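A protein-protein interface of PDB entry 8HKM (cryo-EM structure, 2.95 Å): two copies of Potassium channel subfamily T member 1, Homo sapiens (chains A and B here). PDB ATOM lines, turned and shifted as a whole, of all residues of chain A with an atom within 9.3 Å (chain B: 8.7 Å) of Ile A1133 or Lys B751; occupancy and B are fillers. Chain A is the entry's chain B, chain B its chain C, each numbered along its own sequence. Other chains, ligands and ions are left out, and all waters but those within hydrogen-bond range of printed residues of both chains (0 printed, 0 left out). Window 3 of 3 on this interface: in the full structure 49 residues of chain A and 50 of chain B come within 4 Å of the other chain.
Among the printed residues, pairs that only touch across the chains: Arg A1137 with Tyr B753, Arg A1137 with Leu B1204, Ile A1133 with Leu B1204, Ile A1133 with Lys B751, Gln A1136 with Tyr B753, Ile A1133 with Leu B766 and Leu A1140 with Tyr B753.
The backbone carbonyl oxygen (O) of Leu B766 is in hydrogen-bond range of the backbone NH (N) of Tyr B824 (2.8 Å).
Of the 13 printed residues of chain A, 4 touch a printed residue of chain B. Among the printed residues, no Asp or Glu carboxylate lies within 4 Å of a Lys or Arg side-chain nitrogen of the other chain.
No position is printed for both chains. Of the 7 pairs that touch across the chains among the printed residues, none has its exchanged pair printed and touching as well.
Of the printed residues of chain B, Gln A1136 touches Tyr B753. Of the printed residues of chain B, Arg A1137 touches Tyr B753 and Leu B1204. No residue of chain A comes within 4 Å of Val B750. Lys B751 touches just one residue of chain A: Ile A1133. No residue of chain A comes within 4 Å of Gly B752. Of the printed residues of chain A, Tyr B753 touches Gln A1136, Arg A1137 and Leu A1140. Printed residues of chain A within 4 Å of Leu B1204: Ile A1133 (3.7 Å) and Arg A1137 (3.3 Å). The nearest residue of chain B that does not touch Ile A1133 is Tyr B753 (4.8 Å).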
ATOM      1  N   ALA A1128      13.322   2.837  21.442  1.00  0.00           N
ATOM      2  CA  ALA A1128      12.704   1.969  22.437  1.00  0.00           C
ATOM      3  C   ALA A1128      11.904   2.784  23.447  1.00  0.00           C
ATOM      4  O   ALA A1128      11.221   2.228  24.307  1.00  0.00           O
ATOM      5  CB  ALA A1128      13.761   1.135  23.145  1.00  0.00           C
ATOM      6  N   ALA A1129      11.995   4.112  23.337  1.00  0.00           N
ATOM      7  CA  ALA A1129      11.255   4.988  24.237  1.00  0.00           C
ATOM      8  C   ALA A1129       9.756   4.960  23.971  1.00  0.00           C
ATOM      9  O   ALA A1129       8.979   5.369  24.841  1.00  0.00           O
ATOM     10  CB  ALA A1129      11.777   6.421  24.125  1.00  0.00           C
ATOM     11  N   ALA A1130       9.336   4.494  22.793  1.00  0.00           N
ATOM     12  CA  ALA A1130       7.911   4.425  22.487  1.00  0.00           C
ATOM     13  C   ALA A1130       7.190   3.432  23.389  1.00  0.00           C
ATOM     14  O   ALA A1130       6.019   3.640  23.728  1.00  0.00           O
ATOM     15  CB  ALA A1130       7.705   4.056  21.018  1.00  0.00           C
ATOM     16  N   GLU A1131       7.863   2.344  23.777  1.00  0.00           N
ATOM     17  CA  GLU A1131       7.240   1.366  24.662  1.00  0.00           C
ATOM     18  C   GLU A1131       6.877   1.988  26.005  1.00  0.00           C
ATOM     19  O   GLU A1131       5.779   1.759  26.527  1.00  0.00           O
ATOM     20  CB  GLU A1131       8.166   0.166  24.855  1.00  0.00           C
ATOM     21  CG  GLU A1131       8.324  -0.698  23.613  1.00  0.00           C
ATOM     22  CD  GLU A1131       9.360  -1.790  23.789  1.00  0.00           C
ATOM     23  OE1 GLU A1131      10.115  -1.742  24.783  1.00  0.00           O
ATOM     24  OE2 GLU A1131       9.418  -2.698  22.934  1.00  0.00           O
ATOM     25  N   TRP A1132       7.787   2.777  26.582  1.00  0.00           N
ATOM     26  CA  TRP A1132       7.458   3.509  27.801  1.00  0.00           C
ATOM     27  C   TRP A1132       6.379   4.551  27.539  1.00  0.00           C
ATOM     28  O   TRP A1132       5.503   4.775  28.382  1.00  0.00           O
ATOM     29  CB  TRP A1132       8.713   4.164  28.379  1.00  0.00           C
ATOM     30  CG  TRP A1132       8.455   4.953  29.628  1.00  0.00           C
ATOM     31  CD1 TRP A1132       8.411   4.477  30.905  1.00  0.00           C
ATOM     32  CD2 TRP A1132       8.213   6.363  29.718  1.00  0.00           C
ATOM     33  NE1 TRP A1132       8.151   5.499  31.784  1.00  0.00           N
ATOM     34  CE2 TRP A1132       8.027   6.669  31.081  1.00  0.00           C
ATOM     35  CE3 TRP A1132       8.133   7.395  28.779  1.00  0.00           C
ATOM     36  CZ2 TRP A1132       7.767   7.962  31.527  1.00  0.00           C
ATOM     37  CZ3 TRP A1132       7.876   8.679  29.224  1.00  0.00           C
ATOM     38  CH2 TRP A1132       7.696   8.951  30.585  1.00  0.00           C
ATOM     39  N   ILE A1133       6.434   5.205  26.375  1.00  0.00           N
ATOM     40  CA  ILE A1133       5.385   6.148  25.999  1.00  0.00           C
ATOM     41  C   ILE A1133       4.049   5.428  25.871  1.00  0.00           C
ATOM     42  O   ILE A1133       3.012   5.921  26.334  1.00  0.00           O
ATOM     43  CB  ILE A1133       5.768   6.877  24.697  1.00  0.00           C
ATOM     44  CG1 ILE A1133       6.889   7.885  24.957  1.00  0.00           C
ATOM     45  CG2 ILE A1133       4.562   7.580  24.098  1.00  0.00           C
ATOM     46  CD1 ILE A1133       6.509   8.986  25.921  1.00  0.00           C
ATOM     47  N   SER A1134       4.050   4.248  25.246  1.00  0.00           N
ATOM     48  CA  SER A1134       2.824   3.468  25.141  1.00  0.00           C
ATOM     49  C   SER A1134       2.442   2.833  26.474  1.00  0.00           C
ATOM     50  O   SER A1134       1.263   2.542  26.703  1.00  0.00           O
ATOM     51  CB  SER A1134       2.974   2.392  24.065  1.00  0.00           C
ATOM     52  OG  SER A1134       3.941   1.426  24.438  1.00  0.00           O
ATOM     53  N   GLN A1135       3.419   2.601  27.354  1.00  0.00           N
ATOM     54  CA  GLN A1135       3.121   2.007  28.654  1.00  0.00           C
ATOM     55  C   GLN A1135       2.240   2.928  29.489  1.00  0.00           C
ATOM     56  O   GLN A1135       1.228   2.496  30.054  1.00  0.00           O
ATOM     57  CB  GLN A1135       4.419   1.684  29.396  1.00  0.00           C
ATOM     58  N   GLN A1136       2.614   4.206  29.585  1.00  0.00           N
ATOM     59  CA  GLN A1136       1.801   5.154  30.339  1.00  0.00           C
ATOM     60  C   GLN A1136       0.483   5.451  29.635  1.00  0.00           C
ATOM     61  O   GLN A1136      -0.494   5.828  30.291  1.00  0.00           O
ATOM     62  CB  GLN A1136       2.576   6.451  30.578  1.00  0.00           C
ATOM     63  CG  GLN A1136       3.003   7.167  29.308  1.00  0.00           C
ATOM     64  CD  GLN A1136       4.104   8.179  29.552  1.00  0.00           C
ATOM     65  OE1 GLN A1136       4.569   8.845  28.626  1.00  0.00           O
ATOM     66  NE2 GLN A1136       4.524   8.306  30.806  1.00  0.00           N
ATOM     67  N   ARG A1137       0.441   5.298  28.310  1.00  0.00           N
ATOM     68  CA  ARG A1137      -0.782   5.591  27.570  1.00  0.00           C
ATOM     69  C   ARG A1137      -1.912   4.652  27.971  1.00  0.00           C
ATOM     70  O   ARG A1137      -3.052   5.089  28.169  1.00  0.00           O
ATOM     71  CB  ARG A1137      -0.524   5.501  26.067  1.00  0.00           C
ATOM     72  CG  ARG A1137      -1.716   5.898  25.216  1.00  0.00           C
ATOM     73  CD  ARG A1137      -1.281   6.616  23.952  1.00  0.00           C
ATOM     74  NE  ARG A1137      -2.291   6.529  22.906  1.00  0.00           N
ATOM     75  CZ  ARG A1137      -2.395   5.526  22.046  1.00  0.00           C
ATOM     76  NH1 ARG A1137      -1.566   4.495  22.084  1.00  0.00           N
ATOM     77  NH2 ARG A1137      -3.357   5.554  21.130  1.00  0.00           N
ATOM     78  N   LEU A1138      -1.617   3.358  28.095  1.00  0.00           N
ATOM     79  CA  LEU A1138      -2.635   2.403  28.508  1.00  0.00           C
ATOM     80  C   LEU A1138      -2.999   2.550  29.979  1.00  0.00           C
ATOM     81  O   LEU A1138      -4.143   2.271  30.351  1.00  0.00           O
ATOM     82  CB  LEU A1138      -2.160   0.977  28.226  1.00  0.00           C
ATOM     83  CG  LEU A1138      -3.221  -0.001  27.722  1.00  0.00           C
ATOM     84  CD1 LEU A1138      -3.538   0.260  26.258  1.00  0.00           C
ATOM     85  CD2 LEU A1138      -2.770  -1.438  27.928  1.00  0.00           C
ATOM     86  N   SER A1139      -2.057   2.988  30.816  1.00  0.00           N
ATOM     87  CA  SER A1139      -2.340   3.174  32.236  1.00  0.00           C
ATOM     88  C   SER A1139      -3.296   4.338  32.465  1.00  0.00           C
ATOM     89  O   SER A1139      -4.225   4.238  33.273  1.00  0.00           O
ATOM     90  CB  SER A1139      -1.036   3.391  33.005  1.00  0.00           C
ATOM     91  OG  SER A1139      -1.284   3.594  34.385  1.00  0.00           O
ATOM     92  N   LEU A1140      -3.080   5.453  31.763  1.00  0.00           N
ATOM     93  CA  LEU A1140      -3.959   6.607  31.921  1.00  0.00           C
ATOM     94  C   LEU A1140      -5.353   6.329  31.373  1.00  0.00           C
ATOM     95  O   LEU A1140      -6.340   6.858  31.898  1.00  0.00           O
ATOM     96  CB  LEU A1140      -3.352   7.833  31.236  1.00  0.00           C
ATOM     97  CG  LEU A1140      -2.015   8.369  31.761  1.00  0.00           C
ATOM     98  CD1 LEU A1140      -1.940   9.875  31.583  1.00  0.00           C
ATOM     99  CD2 LEU A1140      -1.794   8.004  33.223  1.00  0.00           C
ATOM    100  N   GLU B 748      14.485  21.798  21.920  1.00  0.00           N
ATOM    101  CA  GLU B 748      13.889  20.519  21.561  1.00  0.00           C
ATOM    102  C   GLU B 748      12.745  20.202  22.514  1.00  0.00           C
ATOM    103  O   GLU B 748      12.921  20.232  23.736  1.00  0.00           O
ATOM    104  CB  GLU B 748      14.937  19.405  21.596  1.00  0.00           C
ATOM    105  CG  GLU B 748      15.616  19.136  20.260  1.00  0.00           C
ATOM    106  CD  GLU B 748      16.096  20.401  19.571  1.00  0.00           C
ATOM    107  OE1 GLU B 748      16.719  21.251  20.245  1.00  0.00           O
ATOM    108  OE2 GLU B 748      15.850  20.546  18.356  1.00  0.00           O
ATOM    109  N   TYR B 749      11.577  19.900  21.953  1.00  0.00           N
ATOM    110  CA  TYR B 749      10.386  19.632  22.745  1.00  0.00           C
ATOM    111  C   TYR B 749      10.272  18.146  23.050  1.00  0.00           C
ATOM    112  O   TYR B 749      10.492  17.300  22.178  1.00  0.00           O
ATOM    113  CB  TYR B 749       9.132  20.108  22.011  1.00  0.00           C
ATOM    114  CG  TYR B 749       9.147  21.576  21.657  1.00  0.00           C
ATOM    115  CD1 TYR B 749       9.696  22.514  22.521  1.00  0.00           C
ATOM    116  CD2 TYR B 749       8.615  22.026  20.458  1.00  0.00           C
ATOM    117  CE1 TYR B 749       9.713  23.857  22.200  1.00  0.00           C
ATOM    118  CE2 TYR B 749       8.628  23.366  20.127  1.00  0.00           C
ATOM    119  CZ  TYR B 749       9.178  24.277  21.002  1.00  0.00           C
ATOM    120  OH  TYR B 749       9.192  25.614  20.677  1.00  0.00           O
ATOM    121  N   VAL B 750       9.926  17.833  24.293  1.00  0.00           N
ATOM    122  CA  VAL B 750       9.720  16.455  24.707  1.00  0.00           C
ATOM    123  C   VAL B 750       8.263  16.079  24.473  1.00  0.00           C
ATOM    124  O   VAL B 750       7.376  16.933  24.394  1.00  0.00           O
ATOM    125  CB  VAL B 750      10.122  16.238  26.179  1.00  0.00           C
ATOM    126  CG1 VAL B 750      11.586  16.588  26.387  1.00  0.00           C
ATOM    127  CG2 VAL B 750       9.234  17.062  27.100  1.00  0.00           C
ATOM    128  N   LYS B 751       8.011  14.779  24.359  1.00  0.00           N
ATOM    129  CA  LYS B 751       6.668  14.248  24.174  1.00  0.00           C
ATOM    130  C   LYS B 751       6.208  13.616  25.480  1.00  0.00           C
ATOM    131  O   LYS B 751       6.823  12.658  25.961  1.00  0.00           O
ATOM    132  CB  LYS B 751       6.628  13.228  23.035  1.00  0.00           C
ATOM    133  CG  LYS B 751       6.827  13.832  21.655  1.00  0.00           C
ATOM    134  CD  LYS B 751       6.702  12.778  20.567  1.00  0.00           C
ATOM    135  CE  LYS B 751       6.947  13.375  19.192  1.00  0.00           C
ATOM    136  NZ  LYS B 751       6.984  12.332  18.130  1.00  0.00           N
ATOM    137  N   GLY B 752       5.130  14.151  26.046  1.00  0.00           N
ATOM    138  CA  GLY B 752       4.600  13.639  27.296  1.00  0.00           C
ATOM    139  C   GLY B 752       3.252  14.256  27.592  1.00  0.00           C
ATOM    140  O   GLY B 752       2.824  15.218  26.950  1.00  0.00           O
ATOM    141  N   TYR B 753       2.581  13.678  28.579  1.00  0.00           N
ATOM    142  CA  TYR B 753       1.276  14.180  28.981  1.00  0.00           C
ATOM    143  C   TYR B 753       1.430  15.458  29.803  1.00  0.00           C
ATOM    144  O   TYR B 753       2.381  15.584  30.579  1.00  0.00           O
ATOM    145  CB  TYR B 753       0.524  13.128  29.788  1.00  0.00           C
ATOM    146  CG  TYR B 753       0.117  11.931  28.967  1.00  0.00           C
ATOM    147  CD1 TYR B 753      -1.105  11.900  28.314  1.00  0.00           C
ATOM    148  CD2 TYR B 753       0.957  10.834  28.839  1.00  0.00           C
ATOM    149  CE1 TYR B 753      -1.482  10.811  27.560  1.00  0.00           C
ATOM    150  CE2 TYR B 753       0.587   9.737  28.085  1.00  0.00           C
ATOM    151  CZ  TYR B 753      -0.634   9.734  27.448  1.00  0.00           C
ATOM    152  OH  TYR B 753      -1.013   8.651  26.695  1.00  0.00           O
ATOM    153  N   PRO B 754       0.523  16.419  29.644  1.00  0.00           N
ATOM    154  CA  PRO B 754       0.584  17.642  30.451  1.00  0.00           C
ATOM    155  C   PRO B 754       0.463  17.322  31.930  1.00  0.00           C
ATOM    156  O   PRO B 754      -0.331  16.455  32.325  1.00  0.00           O
ATOM    157  CB  PRO B 754      -0.621  18.456  29.952  1.00  0.00           C
ATOM    158  CG  PRO B 754      -0.926  17.893  28.599  1.00  0.00           C
ATOM    159  CD  PRO B 754      -0.604  16.437  28.698  1.00  0.00           C
ATOM    160  N   THR B 765      -4.075  13.621  26.580  1.00  0.00           N
ATOM    161  CA  THR B 765      -3.571  13.519  25.220  1.00  0.00           C
ATOM    162  C   THR B 765      -2.072  13.781  25.213  1.00  0.00           C
ATOM    163  O   THR B 765      -1.597  14.737  25.833  1.00  0.00           O
ATOM    164  CB  THR B 765      -4.278  14.511  24.290  1.00  0.00           C
ATOM    165  OG1 THR B 765      -5.695  14.430  24.489  1.00  0.00           O
ATOM    166  CG2 THR B 765      -3.957  14.201  22.835  1.00  0.00           C
ATOM    167  N   LEU B 766      -1.330  12.920  24.521  1.00  0.00           N
ATOM    168  CA  LEU B 766       0.113  13.092  24.411  1.00  0.00           C
ATOM    169  C   LEU B 766       0.414  14.329  23.574  1.00  0.00           C
ATOM    170  O   LEU B 766       0.077  14.382  22.387  1.00  0.00           O
ATOM    171  CB  LEU B 766       0.748  11.850  23.790  1.00  0.00           C
ATOM    172  CG  LEU B 766       2.254  11.685  23.990  1.00  0.00           C
ATOM    173  CD1 LEU B 766       2.557  11.241  25.410  1.00  0.00           C
ATOM    174  CD2 LEU B 766       2.824  10.698  22.984  1.00  0.00           C
ATOM    175  N   CYS B 767       1.043  15.325  24.191  1.00  0.00           N
ATOM    176  CA  CYS B 767       1.283  16.607  23.554  1.00  0.00           C
ATOM    177  C   CYS B 767       2.761  16.971  23.607  1.00  0.00           C
ATOM    178  O   CYS B 767       3.516  16.485  24.454  1.00  0.00           O
ATOM    179  CB  CYS B 767       0.461  17.720  24.219  1.00  0.00           C
ATOM    180  SG  CYS B 767      -1.320  17.435  24.222  1.00  0.00           S
ATOM    181  N   HIS B 768       3.165  17.832  22.676  1.00  0.00           N
ATOM    182  CA  HIS B 768       4.490  18.430  22.735  1.00  0.00           C
ATOM    183  C   HIS B 768       4.592  19.298  23.981  1.00  0.00           C
ATOM    184  O   HIS B 768       3.678  20.070  24.287  1.00  0.00           O
ATOM    185  CB  HIS B 768       4.755  19.264  21.484  1.00  0.00           C
ATOM    186  CG  HIS B 768       4.708  18.478  20.210  1.00  0.00           C
ATOM    187  ND1 HIS B 768       5.662  17.540  19.879  1.00  0.00           N
ATOM    188  CD2 HIS B 768       3.825  18.496  19.185  1.00  0.00           C
ATOM    189  CE1 HIS B 768       5.366  17.011  18.705  1.00  0.00           C
ATOM    190  NE2 HIS B 768       4.256  17.573  18.262  1.00  0.00           N
ATOM    191  N   LEU B 769       5.699  19.169  24.707  1.00  0.00           N
ATOM    192  CA  LEU B 769       5.877  19.874  25.966  1.00  0.00           C
ATOM    193  C   LEU B 769       7.266  20.490  26.033  1.00  0.00           C
ATOM    194  O   LEU B 769       8.230  19.956  25.481  1.00  0.00           O
ATOM    195  CB  LEU B 769       5.671  18.942  27.166  1.00  0.00           C
ATOM    196  CG  LEU B 769       4.256  18.419  27.413  1.00  0.00           C
ATOM    197  CD1 LEU B 769       4.221  17.573  28.675  1.00  0.00           C
ATOM    198  CD2 LEU B 769       3.262  19.564  27.502  1.00  0.00           C
ATOM    199  N   LEU B 770       7.351  21.626  26.717  1.00  0.00           N
ATOM    200  CA  LEU B 770       8.644  22.223  27.002  1.00  0.00           C
ATOM    201  C   LEU B 770       9.410  21.347  27.991  1.00  0.00           C
ATOM    202  O   LEU B 770       8.804  20.738  28.879  1.00  0.00           O
ATOM    203  CB  LEU B 770       8.471  23.629  27.575  1.00  0.00           C
ATOM    204  CG  LEU B 770       8.020  24.725  26.608  1.00  0.00           C
ATOM    205  CD1 LEU B 770       7.682  25.997  27.368  1.00  0.00           C
ATOM    206  CD2 LEU B 770       9.089  24.994  25.563  1.00  0.00           C
ATOM    207  N   PRO B 771      10.736  21.248  27.857  1.00  0.00           N
ATOM    208  CA  PRO B 771      11.509  20.464  28.835  1.00  0.00           C
ATOM    209  C   PRO B 771      11.360  20.971  30.258  1.00  0.00           C
ATOM    210  O   PRO B 771      11.370  20.168  31.199  1.00  0.00           O
ATOM    211  CB  PRO B 771      12.953  20.605  28.332  1.00  0.00           C
ATOM    212  CG  PRO B 771      12.821  20.960  26.886  1.00  0.00           C
ATOM    213  CD  PRO B 771      11.589  21.806  26.796  1.00  0.00           C
ATOM    214  N   ARG B 822      -1.351  21.153  19.906  1.00  0.00           N
ATOM    215  CA  ARG B 822      -0.068  20.728  20.449  1.00  0.00           C
ATOM    216  C   ARG B 822       0.048  19.216  20.588  1.00  0.00           C
ATOM    217  O   ARG B 822       0.980  18.739  21.243  1.00  0.00           O
ATOM    218  CB  ARG B 822       0.177  21.397  21.804  1.00  0.00           C
ATOM    219  CG  ARG B 822       0.329  22.904  21.722  1.00  0.00           C
ATOM    220  CD  ARG B 822       1.462  23.281  20.785  1.00  0.00           C
ATOM    221  NE  ARG B 822       1.874  24.669  20.952  1.00  0.00           N
ATOM    222  CZ  ARG B 822       1.525  25.654  20.136  1.00  0.00           C
ATOM    223  NH1 ARG B 822       0.767  25.434  19.075  1.00  0.00           N
ATOM    224  NH2 ARG B 822       1.950  26.887  20.390  1.00  0.00           N
ATOM    225  N   ALA B 823      -0.861  18.453  19.986  1.00  0.00           N
ATOM    226  CA  ALA B 823      -0.824  17.005  20.106  1.00  0.00           C
ATOM    227  C   ALA B 823       0.422  16.439  19.430  1.00  0.00           C
ATOM    228  O   ALA B 823       1.025  17.060  18.551  1.00  0.00           O
ATOM    229  CB  ALA B 823      -2.082  16.385  19.501  1.00  0.00           C
ATOM    230  N   TYR B 824       0.808  15.234  19.858  1.00  0.00           N
ATOM    231  CA  TYR B 824       2.088  14.676  19.431  1.00  0.00           C
ATOM    232  C   TYR B 824       2.085  14.299  17.955  1.00  0.00           C
ATOM    233  O   TYR B 824       3.141  14.326  17.314  1.00  0.00           O
ATOM    234  CB  TYR B 824       2.452  13.463  20.288  1.00  0.00           C
ATOM    235  CG  TYR B 824       1.738  12.185  19.908  1.00  0.00           C
ATOM    236  CD1 TYR B 824       0.420  11.962  20.280  1.00  0.00           C
ATOM    237  CD2 TYR B 824       2.389  11.195  19.182  1.00  0.00           C
ATOM    238  CE1 TYR B 824      -0.232  10.793  19.937  1.00  0.00           C
ATOM    239  CE2 TYR B 824       1.746  10.025  18.834  1.00  0.00           C
ATOM    240  CZ  TYR B 824       0.435   9.828  19.213  1.00  0.00           C
ATOM    241  OH  TYR B 824      -0.207   8.663  18.869  1.00  0.00           O
ATOM    242  N   TYR B 825       0.927  13.947  17.395  1.00  0.00           N
ATOM    243  CA  TYR B 825       0.889  13.596  15.982  1.00  0.00           C
ATOM    244  C   TYR B 825       0.907  14.818  15.074  1.00  0.00           C
ATOM    245  O   TYR B 825       1.087  14.664  13.861  1.00  0.00           O
ATOM    246  CB  TYR B 825      -0.336  12.732  15.666  1.00  0.00           C
ATOM    247  CG  TYR B 825      -1.587  13.075  16.444  1.00  0.00           C
ATOM    248  CD1 TYR B 825      -2.277  14.253  16.201  1.00  0.00           C
ATOM    249  CD2 TYR B 825      -2.086  12.212  17.409  1.00  0.00           C
ATOM    250  CE1 TYR B 825      -3.427  14.564  16.902  1.00  0.00           C
ATOM    251  CE2 TYR B 825      -3.232  12.517  18.117  1.00  0.00           C
ATOM    252  CZ  TYR B 825      -3.898  13.695  17.860  1.00  0.00           C
ATOM    253  OH  TYR B 825      -5.040  14.002  18.563  1.00  0.00           O
ATOM    254  N   ARG B 826       0.725  16.017  15.621  1.00  0.00           N
ATOM    255  CA  ARG B 826       0.940  17.229  14.851  1.00  0.00           C
ATOM    256  C   ARG B 826       2.429  17.411  14.565  1.00  0.00           C
ATOM    257  O   ARG B 826       3.295  16.927  15.299  1.00  0.00           O
ATOM    258  CB  ARG B 826       0.401  18.451  15.597  1.00  0.00           C
ATOM    259  CG  ARG B 826      -1.041  18.334  16.062  1.00  0.00           C
ATOM    260  CD  ARG B 826      -1.975  17.961  14.921  1.00  0.00           C
ATOM    261  NE  ARG B 826      -3.313  17.639  15.403  1.00  0.00           N
ATOM    262  CZ  ARG B 826      -4.243  17.027  14.683  1.00  0.00           C
ATOM    263  NH1 ARG B 826      -4.018  16.657  13.432  1.00  0.00           N
ATOM    264  NH2 ARG B 826      -5.428  16.780  15.232  1.00  0.00           N
ATOM    265  N   SER B 827       2.721  18.123  13.481  1.00  0.00           N
ATOM    266  CA  SER B 827       4.104  18.336  13.083  1.00  0.00           C
ATOM    267  C   SER B 827       4.791  19.325  14.016  1.00  0.00           C
ATOM    268  O   SER B 827       4.237  20.375  14.354  1.00  0.00           O
ATOM    269  CB  SER B 827       4.170  18.840  11.643  1.00  0.00           C
ATOM    270  OG  SER B 827       5.480  19.262  11.312  1.00  0.00           O
ATOM    271  N   ARG B 828       6.012  18.981  14.433  1.00  0.00           N
ATOM    272  CA  ARG B 828       6.791  19.885  15.274  1.00  0.00           C
ATOM    273  C   ARG B 828       7.163  21.148  14.507  1.00  0.00           C
ATOM    274  O   ARG B 828       7.026  22.261  15.027  1.00  0.00           O
ATOM    275  CB  ARG B 828       8.038  19.156  15.791  1.00  0.00           C
ATOM    276  CG  ARG B 828       8.984  19.941  16.722  1.00  0.00           C
ATOM    277  CD  ARG B 828      10.161  19.130  17.253  1.00  0.00           C
ATOM    278  NE  ARG B 828      11.077  18.717  16.196  1.00  0.00           N
ATOM    279  CZ  ARG B 828      12.038  19.483  15.700  1.00  0.00           C
ATOM    280  NH1 ARG B 828      12.235  20.716  16.138  1.00  0.00           N
ATOM    281  NH2 ARG B 828      12.823  19.002  14.740  1.00  0.00           N
ATOM    282  N   PRO B1203      -0.553   6.423  15.525  1.00  0.00           N
ATOM    283  CA  PRO B1203       0.873   6.085  15.386  1.00  0.00           C
ATOM    284  C   PRO B1203       1.363   5.081  16.413  1.00  0.00           C
ATOM    285  O   PRO B1203       2.267   4.290  16.112  1.00  0.00           O
ATOM    286  CB  PRO B1203       1.572   7.443  15.546  1.00  0.00           C
ATOM    287  CG  PRO B1203       0.524   8.457  15.214  1.00  0.00           C
ATOM    288  CD  PRO B1203      -0.768   7.870  15.692  1.00  0.00           C
ATOM    289  N   LEU B1204       0.799   5.087  17.617  1.00  0.00           N
ATOM    290  CA  LEU B1204       1.253   4.226  18.700  1.00  0.00           C
ATOM    291  C   LEU B1204       0.583   2.857  18.693  1.00  0.00           C
ATOM    292  O   LEU B1204       0.877   2.034  19.565  1.00  0.00           O
ATOM    293  CB  LEU B1204       1.017   4.911  20.048  1.00  0.00           C
ATOM    294  CG  LEU B1204       1.798   6.198  20.328  1.00  0.00           C
ATOM    295  CD1 LEU B1204       1.948   6.409  21.825  1.00  0.00           C
ATOM    296  CD2 LEU B1204       3.162   6.174  19.651  1.00  0.00           C
